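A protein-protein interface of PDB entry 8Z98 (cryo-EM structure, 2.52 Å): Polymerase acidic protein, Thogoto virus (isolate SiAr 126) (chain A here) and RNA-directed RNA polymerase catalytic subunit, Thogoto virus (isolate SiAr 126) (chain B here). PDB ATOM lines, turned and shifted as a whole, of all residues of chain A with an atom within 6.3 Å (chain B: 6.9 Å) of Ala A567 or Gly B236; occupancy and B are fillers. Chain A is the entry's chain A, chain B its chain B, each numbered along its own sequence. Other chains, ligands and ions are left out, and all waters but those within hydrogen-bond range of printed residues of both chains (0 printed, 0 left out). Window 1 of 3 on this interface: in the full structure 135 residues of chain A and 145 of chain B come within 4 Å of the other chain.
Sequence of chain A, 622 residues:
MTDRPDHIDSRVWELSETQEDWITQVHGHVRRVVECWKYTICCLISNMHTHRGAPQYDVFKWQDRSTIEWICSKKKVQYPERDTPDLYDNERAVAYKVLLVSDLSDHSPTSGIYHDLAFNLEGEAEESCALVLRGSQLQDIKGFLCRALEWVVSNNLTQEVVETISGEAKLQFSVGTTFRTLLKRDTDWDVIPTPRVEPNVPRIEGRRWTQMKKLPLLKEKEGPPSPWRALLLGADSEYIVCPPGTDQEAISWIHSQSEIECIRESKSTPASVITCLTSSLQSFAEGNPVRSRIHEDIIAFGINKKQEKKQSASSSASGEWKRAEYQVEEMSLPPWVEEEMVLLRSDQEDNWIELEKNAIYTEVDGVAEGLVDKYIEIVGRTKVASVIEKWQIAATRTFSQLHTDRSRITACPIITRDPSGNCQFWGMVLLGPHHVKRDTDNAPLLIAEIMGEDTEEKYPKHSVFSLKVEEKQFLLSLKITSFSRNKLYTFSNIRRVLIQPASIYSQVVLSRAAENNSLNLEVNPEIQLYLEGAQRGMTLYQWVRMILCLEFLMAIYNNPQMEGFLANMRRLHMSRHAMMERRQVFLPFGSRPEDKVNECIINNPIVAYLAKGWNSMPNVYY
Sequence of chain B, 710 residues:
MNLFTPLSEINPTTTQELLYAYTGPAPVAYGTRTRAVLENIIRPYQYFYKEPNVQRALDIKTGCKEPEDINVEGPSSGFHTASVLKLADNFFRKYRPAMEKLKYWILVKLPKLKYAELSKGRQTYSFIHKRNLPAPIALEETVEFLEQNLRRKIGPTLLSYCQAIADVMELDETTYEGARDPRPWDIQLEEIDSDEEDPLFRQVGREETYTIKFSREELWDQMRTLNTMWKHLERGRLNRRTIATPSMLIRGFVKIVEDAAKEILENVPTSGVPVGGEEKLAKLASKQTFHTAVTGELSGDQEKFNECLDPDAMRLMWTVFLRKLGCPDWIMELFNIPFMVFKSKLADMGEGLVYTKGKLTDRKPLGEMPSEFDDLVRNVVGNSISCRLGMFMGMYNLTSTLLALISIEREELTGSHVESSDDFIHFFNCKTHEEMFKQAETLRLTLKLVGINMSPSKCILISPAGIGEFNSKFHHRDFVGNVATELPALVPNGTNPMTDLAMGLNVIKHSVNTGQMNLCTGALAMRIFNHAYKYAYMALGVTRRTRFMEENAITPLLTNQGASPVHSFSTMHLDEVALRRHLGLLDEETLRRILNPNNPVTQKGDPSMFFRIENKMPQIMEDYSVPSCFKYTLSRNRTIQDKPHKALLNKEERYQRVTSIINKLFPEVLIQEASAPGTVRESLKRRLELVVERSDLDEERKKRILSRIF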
ATOM      1  N   PRO A 560      10.729 -19.478 -21.338  1.00  0.00           N
ATOM      2  CA  PRO A 560      11.032 -19.706 -19.914  1.00  0.00           C
ATOM      3  C   PRO A 560       9.983 -19.151 -18.967  1.00  0.00           C
ATOM      4  O   PRO A 560       9.700 -19.774 -17.933  1.00  0.00           O
ATOM      5  CB  PRO A 560      12.386 -19.010 -19.739  1.00  0.00           C
ATOM      6  CG  PRO A 560      13.020 -19.141 -21.064  1.00  0.00           C
ATOM      7  CD  PRO A 560      11.911 -18.959 -22.053  1.00  0.00           C
ATOM      8  N   MET A 562       6.718 -18.975 -19.485  1.00  0.00           N
ATOM      9  CA  MET A 562       5.560 -19.863 -19.476  1.00  0.00           C
ATOM     10  C   MET A 562       5.833 -21.129 -18.675  1.00  0.00           C
ATOM     11  O   MET A 562       4.985 -21.569 -17.887  1.00  0.00           O
ATOM     12  CB  MET A 562       5.155 -20.208 -20.909  1.00  0.00           C
ATOM     13  CG  MET A 562       4.178 -21.367 -21.021  1.00  0.00           C
ATOM     14  SD  MET A 562       2.464 -20.878 -20.751  1.00  0.00           S
ATOM     15  CE  MET A 562       2.194 -19.804 -22.156  1.00  0.00           C
ATOM     16  N   GLU A 563       7.011 -21.729 -18.855  1.00  0.00           N
ATOM     17  CA  GLU A 563       7.311 -22.966 -18.141  1.00  0.00           C
ATOM     18  C   GLU A 563       7.483 -22.720 -16.649  1.00  0.00           C
ATOM     19  O   GLU A 563       7.008 -23.514 -15.831  1.00  0.00           O
ATOM     20  CB  GLU A 563       8.552 -23.634 -18.722  1.00  0.00           C
ATOM     21  CG  GLU A 563       8.359 -24.149 -20.130  1.00  0.00           C
ATOM     22  CD  GLU A 563       9.606 -24.789 -20.675  1.00  0.00           C
ATOM     23  OE1 GLU A 563      10.646 -24.714 -19.991  1.00  0.00           O
ATOM     24  OE2 GLU A 563       9.550 -25.368 -21.780  1.00  0.00           O
ATOM     25  N   GLY A 564       8.155 -21.629 -16.274  1.00  0.00           N
ATOM     26  CA  GLY A 564       8.235 -21.286 -14.865  1.00  0.00           C
ATOM     27  C   GLY A 564       6.870 -21.035 -14.256  1.00  0.00           C
ATOM     28  O   GLY A 564       6.576 -21.498 -13.149  1.00  0.00           O
ATOM     29  N   PHE A 565       6.011 -20.316 -14.982  1.00  0.00           N
ATOM     30  CA  PHE A 565       4.667 -20.028 -14.497  1.00  0.00           C
ATOM     31  C   PHE A 565       3.882 -21.314 -14.278  1.00  0.00           C
ATOM     32  O   PHE A 565       3.237 -21.488 -13.242  1.00  0.00           O
ATOM     33  CB  PHE A 565       3.954 -19.108 -15.492  1.00  0.00           C
ATOM     34  CG  PHE A 565       2.484 -18.937 -15.229  1.00  0.00           C
ATOM     35  CD1 PHE A 565       2.035 -17.962 -14.358  1.00  0.00           C
ATOM     36  CD2 PHE A 565       1.551 -19.734 -15.871  1.00  0.00           C
ATOM     37  CE1 PHE A 565       0.689 -17.795 -14.119  1.00  0.00           C
ATOM     38  CE2 PHE A 565       0.204 -19.573 -15.631  1.00  0.00           C
ATOM     39  CZ  PHE A 565      -0.227 -18.602 -14.755  1.00  0.00           C
ATOM     40  N   LEU A 566       3.942 -22.237 -15.238  1.00  0.00           N
ATOM     41  CA  LEU A 566       3.201 -23.489 -15.104  1.00  0.00           C
ATOM     42  C   LEU A 566       3.753 -24.346 -13.970  1.00  0.00           C
ATOM     43  O   LEU A 566       2.986 -24.914 -13.177  1.00  0.00           O
ATOM     44  CB  LEU A 566       3.241 -24.256 -16.422  1.00  0.00           C
ATOM     45  CG  LEU A 566       2.368 -23.693 -17.543  1.00  0.00           C
ATOM     46  CD1 LEU A 566       2.695 -24.378 -18.857  1.00  0.00           C
ATOM     47  CD2 LEU A 566       0.895 -23.835 -17.203  1.00  0.00           C
ATOM     48  N   ALA A 567       5.082 -24.446 -13.874  1.00  0.00           N
ATOM     49  CA  ALA A 567       5.695 -25.269 -12.839  1.00  0.00           C
ATOM     50  C   ALA A 567       5.359 -24.748 -11.450  1.00  0.00           C
ATOM     51  O   ALA A 567       5.086 -25.533 -10.534  1.00  0.00           O
ATOM     52  CB  ALA A 567       7.208 -25.320 -13.042  1.00  0.00           C
ATOM     53  N   ASN A 568       5.371 -23.428 -11.271  1.00  0.00           N
ATOM     54  CA  ASN A 568       5.051 -22.859  -9.971  1.00  0.00           C
ATOM     55  C   ASN A 568       3.553 -22.719  -9.734  1.00  0.00           C
ATOM     56  O   ASN A 568       3.143 -22.509  -8.589  1.00  0.00           O
ATOM     57  CB  ASN A 568       5.742 -21.506  -9.825  1.00  0.00           C
ATOM     58  CG  ASN A 568       7.248 -21.629  -9.849  1.00  0.00           C
ATOM     59  OD1 ASN A 568       7.837 -22.310  -9.011  1.00  0.00           O
ATOM     60  ND2 ASN A 568       7.880 -20.984 -10.821  1.00  0.00           N
ATOM     61  N   MET A 569       2.735 -22.831 -10.778  1.00  0.00           N
ATOM     62  CA  MET A 569       1.288 -22.812 -10.637  1.00  0.00           C
ATOM     63  C   MET A 569       0.704 -24.184 -10.359  1.00  0.00           C
ATOM     64  O   MET A 569      -0.439 -24.272  -9.899  1.00  0.00           O
ATOM     65  CB  MET A 569       0.655 -22.224 -11.903  1.00  0.00           C
ATOM     66  CG  MET A 569      -0.847 -22.042 -11.840  1.00  0.00           C
ATOM     67  SD  MET A 569      -1.341 -20.868 -10.578  1.00  0.00           S
ATOM     68  CE  MET A 569      -0.806 -19.360 -11.353  1.00  0.00           C
ATOM     69  N   ARG A 570       1.447 -25.253 -10.642  1.00  0.00           N
ATOM     70  CA  ARG A 570       0.975 -26.577 -10.250  1.00  0.00           C
ATOM     71  C   ARG A 570       0.732 -26.653  -8.745  1.00  0.00           C
ATOM     72  O   ARG A 570      -0.241 -27.270  -8.297  1.00  0.00           O
ATOM     73  CB  ARG A 570       1.971 -27.645 -10.698  1.00  0.00           C
ATOM     74  CG  ARG A 570       2.069 -27.776 -12.206  1.00  0.00           C
ATOM     75  CD  ARG A 570       3.200 -28.691 -12.626  1.00  0.00           C
ATOM     76  NE  ARG A 570       3.672 -28.363 -13.965  1.00  0.00           N
ATOM     77  CZ  ARG A 570       4.939 -28.410 -14.346  1.00  0.00           C
ATOM     78  NH1 ARG A 570       5.897 -28.788 -13.516  1.00  0.00           N
ATOM     79  NH2 ARG A 570       5.255 -28.068 -15.591  1.00  0.00           N
ATOM     80  N   ARG A 571       1.589 -26.005  -7.952  1.00  0.00           N
ATOM     81  CA  ARG A 571       1.414 -26.001  -6.501  1.00  0.00           C
ATOM     82  C   ARG A 571       0.129 -25.288  -6.096  1.00  0.00           C
ATOM     83  O   ARG A 571      -0.624 -25.771  -5.243  1.00  0.00           O
ATOM     84  CB  ARG A 571       2.618 -25.336  -5.837  1.00  0.00           C
ATOM     85  CG  ARG A 571       3.675 -26.293  -5.334  1.00  0.00           C
ATOM     86  CD  ARG A 571       4.762 -25.539  -4.593  1.00  0.00           C
ATOM     87  NE  ARG A 571       5.298 -24.441  -5.388  1.00  0.00           N
ATOM     88  CZ  ARG A 571       6.209 -24.580  -6.340  1.00  0.00           C
ATOM     89  NH1 ARG A 571       6.726 -25.760  -6.637  1.00  0.00           N
ATOM     90  NH2 ARG A 571       6.616 -23.505  -7.010  1.00  0.00           N
ATOM     91  N   LEU B  19      -1.377 -28.417 -17.188  1.00  0.00           N
ATOM     92  CA  LEU B  19      -0.429 -27.367 -16.834  1.00  0.00           C
ATOM     93  C   LEU B  19       0.986 -27.803 -17.178  1.00  0.00           C
ATOM     94  O   LEU B  19       1.888 -27.732 -16.338  1.00  0.00           O
ATOM     95  CB  LEU B  19      -0.526 -27.020 -15.348  1.00  0.00           C
ATOM     96  CG  LEU B  19      -1.910 -27.012 -14.705  1.00  0.00           C
ATOM     97  CD1 LEU B  19      -1.804 -26.663 -13.234  1.00  0.00           C
ATOM     98  CD2 LEU B  19      -2.822 -26.039 -15.418  1.00  0.00           C
ATOM     99  N   PRO B  27      13.381 -24.225 -23.590  1.00  0.00           N
ATOM    100  CA  PRO B  27      14.315 -23.097 -23.532  1.00  0.00           C
ATOM    101  C   PRO B  27      15.750 -23.561 -23.714  1.00  0.00           C
ATOM    102  O   PRO B  27      16.152 -24.615 -23.219  1.00  0.00           O
ATOM    103  CB  PRO B  27      14.085 -22.521 -22.131  1.00  0.00           C
ATOM    104  CG  PRO B  27      12.706 -22.962 -21.770  1.00  0.00           C
ATOM    105  CD  PRO B  27      12.576 -24.330 -22.365  1.00  0.00           C
ATOM    106  N   GLU B 234      16.099 -28.158 -20.461  1.00  0.00           N
ATOM    107  CA  GLU B 234      15.548 -28.195 -19.116  1.00  0.00           C
ATOM    108  C   GLU B 234      14.255 -27.391 -19.080  1.00  0.00           C
ATOM    109  O   GLU B 234      14.230 -26.230 -19.501  1.00  0.00           O
ATOM    110  CB  GLU B 234      16.549 -27.642 -18.102  1.00  0.00           C
ATOM    111  CG  GLU B 234      16.260 -28.041 -16.668  1.00  0.00           C
ATOM    112  CD  GLU B 234      17.091 -27.265 -15.669  1.00  0.00           C
ATOM    113  OE1 GLU B 234      17.716 -26.260 -16.068  1.00  0.00           O
ATOM    114  OE2 GLU B 234      17.123 -27.663 -14.486  1.00  0.00           O
ATOM    115  N   ARG B 235      13.191 -28.008 -18.582  1.00  0.00           N
ATOM    116  CA  ARG B 235      11.875 -27.394 -18.536  1.00  0.00           C
ATOM    117  C   ARG B 235      11.456 -27.144 -17.093  1.00  0.00           C
ATOM    118  O   ARG B 235      12.003 -27.724 -16.152  1.00  0.00           O
ATOM    119  CB  ARG B 235      10.837 -28.276 -19.239  1.00  0.00           C
ATOM    120  CG  ARG B 235      11.172 -28.596 -20.686  1.00  0.00           C
ATOM    121  CD  ARG B 235      10.045 -29.357 -21.363  1.00  0.00           C
ATOM    122  NE  ARG B 235       9.275 -28.505 -22.259  1.00  0.00           N
ATOM    123  CZ  ARG B 235       9.409 -28.489 -23.578  1.00  0.00           C
ATOM    124  NH1 ARG B 235      10.269 -29.281 -24.194  1.00  0.00           N
ATOM    125  NH2 ARG B 235       8.659 -27.658 -24.296  1.00  0.00           N
ATOM    126  N   GLY B 236      10.471 -26.264 -16.932  1.00  0.00           N
ATOM    127  CA  GLY B 236       9.917 -25.979 -15.626  1.00  0.00           C
ATOM    128  C   GLY B 236      10.682 -24.980 -14.791  1.00  0.00           C
ATOM    129  O   GLY B 236      10.411 -24.868 -13.591  1.00  0.00           O
ATOM    130  N   ARG B 237      11.632 -24.253 -15.376  1.00  0.00           N
ATOM    131  CA  ARG B 237      12.409 -23.262 -14.647  1.00  0.00           C
ATOM    132  C   ARG B 237      12.500 -21.979 -15.456  1.00  0.00           C
ATOM    133  O   ARG B 237      12.689 -22.013 -16.675  1.00  0.00           O
ATOM    134  CB  ARG B 237      13.819 -23.774 -14.331  1.00  0.00           C
ATOM    135  CG  ARG B 237      13.850 -25.035 -13.486  1.00  0.00           C
ATOM    136  CD  ARG B 237      15.250 -25.325 -12.980  1.00  0.00           C
ATOM    137  NE  ARG B 237      15.473 -24.770 -11.650  1.00  0.00           N
ATOM    138  CZ  ARG B 237      15.983 -23.569 -11.414  1.00  0.00           C
ATOM    139  NH1 ARG B 237      16.349 -22.767 -12.399  1.00  0.00           N
ATOM    140  NH2 ARG B 237      16.135 -23.166 -10.155  1.00  0.00           N
ATOM    141  N   LEU B 238      12.362 -20.844 -14.767  1.00  0.00           N
ATOM    142  CA  LEU B 238      12.488 -19.553 -15.436  1.00  0.00           C
ATOM    143  C   LEU B 238      13.934 -19.264 -15.816  1.00  0.00           C
ATOM    144  O   LEU B 238      14.201 -18.723 -16.895  1.00  0.00           O
ATOM    145  CB  LEU B 238      11.939 -18.444 -14.538  1.00  0.00           C
ATOM    146  CG  LEU B 238      12.144 -17.008 -15.023  1.00  0.00           C
ATOM    147  CD1 LEU B 238      11.278 -16.717 -16.236  1.00  0.00           C
ATOM    148  CD2 LEU B 238      11.862 -16.020 -13.905  1.00  0.00           C
ATOM    149  N   ASN B 239      14.878 -19.617 -14.950  1.00  0.00           N
ATOM    150  CA  ASN B 239      16.285 -19.300 -15.141  1.00  0.00           C
ATOM    151  C   ASN B 239      17.076 -20.563 -15.449  1.00  0.00           C
ATOM    152  O   ASN B 239      16.818 -21.626 -14.876  1.00  0.00           O
ATOM    153  CB  ASN B 239      16.862 -18.613 -13.901  1.00  0.00           C
ATOM    154  CG  ASN B 239      16.250 -17.251 -13.654  1.00  0.00           C
ATOM    155  OD1 ASN B 239      15.585 -17.031 -12.642  1.00  0.00           O
ATOM    156  ND2 ASN B 239      16.471 -16.326 -14.579  1.00  0.00           N
ATOM    157  N   ARG B 240      18.036 -20.438 -16.360  1.00  0.00           N
ATOM    158  CA  ARG B 240      18.862 -21.572 -16.746  1.00  0.00           C
ATOM    159  C   ARG B 240      19.839 -21.933 -15.631  1.00  0.00           C
ATOM    160  O   ARG B 240      20.286 -21.077 -14.863  1.00  0.00           O
ATOM    161  CB  ARG B 240      19.628 -21.259 -18.031  1.00  0.00           C
ATOM    162  CG  ARG B 240      18.815 -20.531 -19.090  1.00  0.00           C
ATOM    163  CD  ARG B 240      18.022 -21.489 -19.972  1.00  0.00           C
ATOM    164  NE  ARG B 240      16.917 -22.127 -19.265  1.00  0.00           N
ATOM    165  CZ  ARG B 240      15.799 -21.514 -18.903  1.00  0.00           C
ATOM    166  NH1 ARG B 240      15.597 -20.233 -19.162  1.00  0.00           N
ATOM    167  NH2 ARG B 240      14.860 -22.203 -18.261  1.00  0.00           N
ATOM    168  N   LYS B 458       7.906 -23.164  -1.759  1.00  0.00           N
ATOM    169  CA  LYS B 458       7.639 -24.357  -2.550  1.00  0.00           C
ATOM    170  C   LYS B 458       7.172 -25.540  -1.712  1.00  0.00           C
ATOM    171  O   LYS B 458       6.906 -26.606  -2.270  1.00  0.00           O
ATOM    172  CB  LYS B 458       8.888 -24.749  -3.343  1.00  0.00           C
ATOM    173  CG  LYS B 458       9.253 -23.759  -4.433  1.00  0.00           C
ATOM    174  CD  LYS B 458      10.311 -24.318  -5.359  1.00  0.00           C
ATOM    175  CE  LYS B 458      10.664 -23.320  -6.446  1.00  0.00           C
ATOM    176  NZ  LYS B 458      11.634 -23.883  -7.425  1.00  0.00           N
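Pro B27 touches Pro A560.
Pro A560 touches Arg B237 (O to O, 3.9 Å).
Leu B238 touches Pro A560.
Pro A560 touches Arg B240.
Glu A563 touches Pro B27 (OE1 to CD, 3.1 Å).
Glu A563 touches Glu B234 (OE1 to O, 3.9 Å).
Leu B19 touches Leu A566.
Ala A567 touches Gly B236.
Asn A568 touches Lys B458.
Lys B458 touches Arg A571 (O to CD, 3.3 Å).
Of chain B, only Gly B236 comes within 4 Å of Ala A567.
Of chain A, only Glu A563 (3.4 Å) and Ala A567 (3.3 Å) come within 4 Å of Gly B236.
Of the printed residues of chain A, Arg B235 touches Glu A563 (3.2 Å).
Printed residues of chain B within 4 Å of Arg A570: Leu B19 (3.0 Å).
Printed residues of chain A within 4 Å of Glu B234: Glu A563.
Of the printed residues of chain B, Arg A571 touches Lys B458 (3.3 Å).
Of the printed residues of chain A, Pro B27 touches Pro A560 (3.7 Å) and Glu A563 (3.1 Å).
Met A562 touches none of the printed residues of chain B.
The nearest printed residue of chain B that does not touch Arg A570 is Gly B236 (5.1 Å).
The backbone carbonyl oxygen (O) of Gly A564 is in hydrogen-bond range of the side-chain amide nitrogen (ND2) of Asn A568.
The side-chain amide oxygen (OD1) of Asn A568 sits at hydrogen-bond distance from the guanidinium group (NH2) of Arg A571, 2.6 Å away.
NH1 of Arg B237 sits at hydrogen-bond distance from O of Asn B239 (2.8 Å).
O of Arg B237 is in hydrogen-bond range of NH2 of Arg B240.
The guanidinium group (NH1) of Arg B240 lies within hydrogen-bond range of the backbone carbonyl oxygen (O) of Leu B238, 3.1 Å away.
Of the 10 printed residues of chain B, 9 touch a printed residue of chain A.
Hydrophobic or aromatic side chains of chain B that line the printed part of chain A: Leu B19, Pro B27 and Leu B238.
Of the 11 printed residues of chain A, 7 touch a printed residue of chain B.
Hydrophobic or aromatic side chains of chain A that line the printed part of chain B: Pro A560, Leu A566 and Ala A567.
Among the printed residues, 13 pairs touch across the chains.
Among the printed residues, Asp or Glu carboxylates within 4 Å of a Lys or Arg side-chain nitrogen of the other chain: Glu A563 with Arg B235 (3.2 Å).
OE2 of Glu A563 is in salt-bridge range of NE of Arg B235.
The backbone NH (N) of Gly B236 is in hydrogen-bond range of the side-chain carboxylate (OE1) of Glu A563 (3.4 Å).
NE of Arg A570 lies within hydrogen-bond range of O of Leu B19 (3.0 Å).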
